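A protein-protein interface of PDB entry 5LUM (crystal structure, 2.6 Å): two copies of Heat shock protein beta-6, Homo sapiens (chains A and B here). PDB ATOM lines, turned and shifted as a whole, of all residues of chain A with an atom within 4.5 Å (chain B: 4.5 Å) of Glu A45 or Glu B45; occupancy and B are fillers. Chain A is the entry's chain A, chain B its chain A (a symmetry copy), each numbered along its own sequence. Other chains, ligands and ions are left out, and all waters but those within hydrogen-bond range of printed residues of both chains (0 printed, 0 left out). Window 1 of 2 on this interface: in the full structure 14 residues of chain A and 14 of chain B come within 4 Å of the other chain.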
ATOM      1  N   PHE A  12     -12.846   9.207 -32.394  1.00  0.00           N
ATOM      2  CA  PHE A  12     -14.022  10.096 -32.387  1.00  0.00           C
ATOM      3  C   PHE A  12     -14.818  10.120 -33.682  1.00  0.00           C
ATOM      4  O   PHE A  12     -14.244  10.130 -34.775  1.00  0.00           O
ATOM      5  CB  PHE A  12     -13.617  11.535 -32.041  1.00  0.00           C
ATOM      6  CG  PHE A  12     -12.728  11.664 -30.839  1.00  0.00           C
ATOM      7  CD1 PHE A  12     -13.266  11.699 -29.553  1.00  0.00           C
ATOM      8  CD2 PHE A  12     -11.344  11.707 -30.980  1.00  0.00           C
ATOM      9  CE1 PHE A  12     -12.430  11.776 -28.430  1.00  0.00           C
ATOM     10  CE2 PHE A  12     -10.516  11.741 -29.857  1.00  0.00           C
ATOM     11  CZ  PHE A  12     -11.063  11.799 -28.591  1.00  0.00           C
ATOM     12  N   ALA A  30     -12.356  17.515 -29.041  1.00  0.00           N
ATOM     13  CA  ALA A  30     -12.874  16.183 -29.270  1.00  0.00           C
ATOM     14  C   ALA A  30     -13.094  15.512 -27.886  1.00  0.00           C
ATOM     15  O   ALA A  30     -12.315  15.701 -26.946  1.00  0.00           O
ATOM     16  CB  ALA A  30     -11.952  15.394 -30.167  1.00  0.00           C
ATOM     17  N   ARG A  31     -14.235  14.907 -27.736  1.00  0.00           N
ATOM     18  CA  ARG A  31     -14.683  14.241 -26.523  1.00  0.00           C
ATOM     19  C   ARG A  31     -15.623  13.095 -26.834  1.00  0.00           C
ATOM     20  O   ARG A  31     -16.584  13.256 -27.586  1.00  0.00           O
ATOM     21  CB  ARG A  31     -15.418  15.231 -25.587  1.00  0.00           C
ATOM     22  CG  ARG A  31     -15.746  14.611 -24.210  1.00  0.00           C
ATOM     23  CD  ARG A  31     -16.548  15.546 -23.323  1.00  0.00           C
ATOM     24  NE  ARG A  31     -16.995  14.853 -22.120  1.00  0.00           N
ATOM     25  CZ  ARG A  31     -18.114  14.137 -22.033  1.00  0.00           C
ATOM     26  NH1 ARG A  31     -18.941  14.052 -23.072  1.00  0.00           N
ATOM     27  NH2 ARG A  31     -18.419  13.508 -20.907  1.00  0.00           N
ATOM     28  N   ARG A  44     -12.396   9.538 -23.452  1.00  0.00           N
ATOM     29  CA  ARG A  44     -11.254  10.303 -23.990  1.00  0.00           C
ATOM     30  C   ARG A  44     -11.681  11.691 -24.388  1.00  0.00           C
ATOM     31  O   ARG A  44     -12.821  11.912 -24.795  1.00  0.00           O
ATOM     32  CB  ARG A  44     -10.690   9.615 -25.225  1.00  0.00           C
ATOM     33  CG  ARG A  44      -9.920   8.359 -24.927  1.00  0.00           C
ATOM     34  CD  ARG A  44      -9.541   7.781 -26.235  1.00  0.00           C
ATOM     35  NE  ARG A  44      -9.085   6.392 -26.141  1.00  0.00           N
ATOM     36  CZ  ARG A  44      -9.821   5.334 -26.456  1.00  0.00           C
ATOM     37  NH1 ARG A  44     -11.110   5.477 -26.763  1.00  0.00           N
ATOM     38  NH2 ARG A  44      -9.291   4.122 -26.426  1.00  0.00           N
ATOM     39  N   GLU A  45     -10.758  12.632 -24.276  1.00  0.00           N
ATOM     40  CA  GLU A  45     -11.003  14.030 -24.562  1.00  0.00           C
ATOM     41  C   GLU A  45      -9.701  14.733 -24.901  1.00  0.00           C
ATOM     42  O   GLU A  45      -8.687  14.437 -24.309  1.00  0.00           O
ATOM     43  CB  GLU A  45     -11.685  14.618 -23.335  1.00  0.00           C
ATOM     44  CG  GLU A  45     -11.798  16.110 -23.260  1.00  0.00           C
ATOM     45  CD  GLU A  45     -12.694  16.571 -22.139  1.00  0.00           C
ATOM     46  OE1 GLU A  45     -12.978  15.780 -21.208  1.00  0.00           O
ATOM     47  OE2 GLU A  45     -13.159  17.727 -22.228  1.00  0.00           O
ATOM     48  N   PHE A  46      -9.708  15.606 -25.904  1.00  0.00           N
ATOM     49  CA  PHE A  46      -8.533  16.427 -26.246  1.00  0.00           C
ATOM     50  C   PHE A  46      -8.985  17.804 -26.719  1.00  0.00           C
ATOM     51  O   PHE A  46     -10.125  17.994 -27.151  1.00  0.00           O
ATOM     52  CB  PHE A  46      -7.546  15.734 -27.224  1.00  0.00           C
ATOM     53  CG  PHE A  46      -7.897  15.800 -28.698  1.00  0.00           C
ATOM     54  CD1 PHE A  46      -7.699  16.978 -29.430  1.00  0.00           C
ATOM     55  CD2 PHE A  46      -8.414  14.686 -29.360  1.00  0.00           C
ATOM     56  CE1 PHE A  46      -8.057  17.059 -30.770  1.00  0.00           C
ATOM     57  CE2 PHE A  46      -8.719  14.753 -30.713  1.00  0.00           C
ATOM     58  CZ  PHE A  46      -8.572  15.956 -31.400  1.00  0.00           C
ATOM     59  N   HIS A  47      -8.086  18.753 -26.617  1.00  0.00           N
ATOM     60  CA  HIS A  47      -8.264  20.140 -27.010  1.00  0.00           C
ATOM     61  C   HIS A  47      -6.986  20.540 -27.725  1.00  0.00           C
ATOM     62  O   HIS A  47      -5.919  20.501 -27.118  1.00  0.00           O
ATOM     63  CB  HIS A  47      -8.469  21.047 -25.774  1.00  0.00           C
ATOM     64  CG  HIS A  47      -9.447  20.514 -24.764  1.00  0.00           C
ATOM     65  ND1 HIS A  47     -10.710  21.066 -24.640  1.00  0.00           N
ATOM     66  CD2 HIS A  47      -9.329  19.483 -23.874  1.00  0.00           C
ATOM     67  CE1 HIS A  47     -11.305  20.380 -23.672  1.00  0.00           C
ATOM     68  NE2 HIS A  47     -10.519  19.402 -23.198  1.00  0.00           N
ATOM     69  N   PHE B  12       1.644  11.429 -20.313  1.00  0.00           N
ATOM     70  CA  PHE B  12       1.453  11.907 -18.931  1.00  0.00           C
ATOM     71  C   PHE B  12       2.576  11.556 -17.967  1.00  0.00           C
ATOM     72  O   PHE B  12       3.107  10.442 -17.997  1.00  0.00           O
ATOM     73  CB  PHE B  12       0.135  11.380 -18.348  1.00  0.00           C
ATOM     74  CG  PHE B  12      -1.059  11.555 -19.241  1.00  0.00           C
ATOM     75  CD1 PHE B  12      -1.761  12.759 -19.268  1.00  0.00           C
ATOM     76  CD2 PHE B  12      -1.463  10.533 -20.096  1.00  0.00           C
ATOM     77  CE1 PHE B  12      -2.848  12.934 -20.135  1.00  0.00           C
ATOM     78  CE2 PHE B  12      -2.519  10.727 -20.986  1.00  0.00           C
ATOM     79  CZ  PHE B  12      -3.221  11.917 -20.984  1.00  0.00           C
ATOM     80  N   ALA B  30      -6.250  10.519 -16.146  1.00  0.00           N
ATOM     81  CA  ALA B  30      -5.041  11.161 -16.617  1.00  0.00           C
ATOM     82  C   ALA B  30      -5.452  12.462 -17.361  1.00  0.00           C
ATOM     83  O   ALA B  30      -6.472  12.514 -18.056  1.00  0.00           O
ATOM     84  CB  ALA B  30      -4.233  10.221 -17.478  1.00  0.00           C
ATOM     85  N   ARG B  31      -4.766  13.522 -17.049  1.00  0.00           N
ATOM     86  CA  ARG B  31      -4.987  14.857 -17.581  1.00  0.00           C
ATOM     87  C   ARG B  31      -3.703  15.659 -17.620  1.00  0.00           C
ATOM     88  O   ARG B  31      -2.979  15.734 -16.628  1.00  0.00           O
ATOM     89  CB  ARG B  31      -6.018  15.630 -16.725  1.00  0.00           C
ATOM     90  CG  ARG B  31      -6.421  16.980 -17.359  1.00  0.00           C
ATOM     91  CD  ARG B  31      -7.360  17.784 -16.478  1.00  0.00           C
ATOM     92  NE  ARG B  31      -7.558  19.122 -17.026  1.00  0.00           N
ATOM     93  CZ  ARG B  31      -6.763  20.162 -16.784  1.00  0.00           C
ATOM     94  NH1 ARG B  31      -5.730  20.041 -15.955  1.00  0.00           N
ATOM     95  NH2 ARG B  31      -7.000  21.332 -17.360  1.00  0.00           N
ATOM     96  N   ARG B  44      -4.722  17.009 -23.245  1.00  0.00           N
ATOM     97  CA  ARG B  44      -5.254  15.635 -23.327  1.00  0.00           C
ATOM     98  C   ARG B  44      -5.757  15.176 -21.983  1.00  0.00           C
ATOM     99  O   ARG B  44      -5.243  15.580 -20.942  1.00  0.00           O
ATOM    100  CB  ARG B  44      -4.164  14.670 -23.771  1.00  0.00           C
ATOM    101  CG  ARG B  44      -3.797  14.790 -25.225  1.00  0.00           C
ATOM    102  CD  ARG B  44      -2.667  13.862 -25.448  1.00  0.00           C
ATOM    103  NE  ARG B  44      -1.969  14.097 -26.714  1.00  0.00           N
ATOM    104  CZ  ARG B  44      -0.811  14.732 -26.829  1.00  0.00           C
ATOM    105  NH1 ARG B  44      -0.260  15.328 -25.772  1.00  0.00           N
ATOM    106  NH2 ARG B  44      -0.211  14.816 -28.006  1.00  0.00           N
ATOM    107  N   GLU B  45      -6.766  14.322 -22.008  1.00  0.00           N
ATOM    108  CA  GLU B  45      -7.413  13.815 -20.816  1.00  0.00           C
ATOM    109  C   GLU B  45      -8.092  12.490 -21.110  1.00  0.00           C
ATOM    110  O   GLU B  45      -8.639  12.318 -22.177  1.00  0.00           O
ATOM    111  CB  GLU B  45      -8.392  14.886 -20.356  1.00  0.00           C
ATOM    112  CG  GLU B  45      -9.389  14.502 -19.305  1.00  0.00           C
ATOM    113  CD  GLU B  45     -10.139  15.686 -18.753  1.00  0.00           C
ATOM    114  OE1 GLU B  45     -10.146  16.767 -19.390  1.00  0.00           O
ATOM    115  OE2 GLU B  45     -10.684  15.539 -17.639  1.00  0.00           O
ATOM    116  N   PHE B  46      -7.994  11.524 -20.200  1.00  0.00           N
ATOM    117  CA  PHE B  46      -8.705  10.240 -20.329  1.00  0.00           C
ATOM    118  C   PHE B  46      -9.142   9.752 -18.953  1.00  0.00           C
ATOM    119  O   PHE B  46      -8.591  10.150 -17.923  1.00  0.00           O
ATOM    120  CB  PHE B  46      -7.928   9.171 -21.144  1.00  0.00           C
ATOM    121  CG  PHE B  46      -6.864   8.392 -20.393  1.00  0.00           C
ATOM    122  CD1 PHE B  46      -7.217   7.370 -19.504  1.00  0.00           C
ATOM    123  CD2 PHE B  46      -5.510   8.669 -20.581  1.00  0.00           C
ATOM    124  CE1 PHE B  46      -6.250   6.680 -18.782  1.00  0.00           C
ATOM    125  CE2 PHE B  46      -4.543   7.942 -19.901  1.00  0.00           C
ATOM    126  CZ  PHE B  46      -4.926   6.974 -18.974  1.00  0.00           C
ATOM    127  N   HIS B  47     -10.142   8.903 -18.953  1.00  0.00           N
ATOM    128  CA  HIS B  47     -10.733   8.285 -17.778  1.00  0.00           C
ATOM    129  C   HIS B  47     -10.952   6.827 -18.140  1.00  0.00           C
ATOM    130  O   HIS B  47     -11.696   6.543 -19.074  1.00  0.00           O
ATOM    131  CB  HIS B  47     -12.090   8.938 -17.428  1.00  0.00           C
ATOM    132  CG  HIS B  47     -12.084  10.442 -17.452  1.00  0.00           C
ATOM    133  ND1 HIS B  47     -12.102  11.169 -16.275  1.00  0.00           N
ATOM    134  CD2 HIS B  47     -12.041  11.312 -18.506  1.00  0.00           C
ATOM    135  CE1 HIS B  47     -12.096  12.444 -16.644  1.00  0.00           C
ATOM    136  NE2 HIS B  47     -12.036  12.577 -17.977  1.00  0.00           N
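N of Glu A45 sits at hydrogen-bond distance from O of Glu B45, 3.0 Å away.
Arg A44 touches Glu B45, and with the chains exchanged Glu A45 touches Arg B44. Glu A45 touches its own counterpart, Glu B45. Positions printed for both chains: 12, 30, 31, 44, 45, 46 and 47.
The side-chain carboxylate (OE2) of Glu B45 is in hydrogen-bond range of a ring nitrogen (NE2) of His B47 (3.3 Å). The side-chain carboxylate (OE2) of Glu A45 is in hydrogen-bond range of a ring nitrogen (NE2) of His A47 (3.3 Å).
Among the printed residues, merely in contact across the chains: Arg A44 with Glu B45 and Glu A45 with Arg B44.
Of the 7 printed residues of chain A, 2 touch a printed residue of chain B. Printed residues of chain B that touch a printed residue of chain A: Arg B44 and Glu B45. Along chain B the printed residues that touch a printed residue of chain A span positions 44 to 45. Among the printed residues, no Asp or Glu carboxylate lies within 4 Å of a Lys or Arg side-chain nitrogen of the other chain.
Of chain B, only Arg B44 (3.8 Å) and Glu B45 (3.0 Å) come within 4 Å of Glu A45. Of chain A, only Arg A44 and Glu A45 come within 4 Å of Glu B45. Of the printed residues of chain A, Arg B44 touches Glu A45 (3.8 Å). Of the printed residues of chain B, Arg A44 touches Glu B45 (3.8 Å). Ala B30 touches none of the printed residues of chain A. His A47 touches none of the printed residues of chain B. The nearest printed residue of chain B that does not touch Glu A45 is His B47 (4.6 Å). The nearest printed residue of chain A that does not touch Glu B45 is His A47 (4.6 Å).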
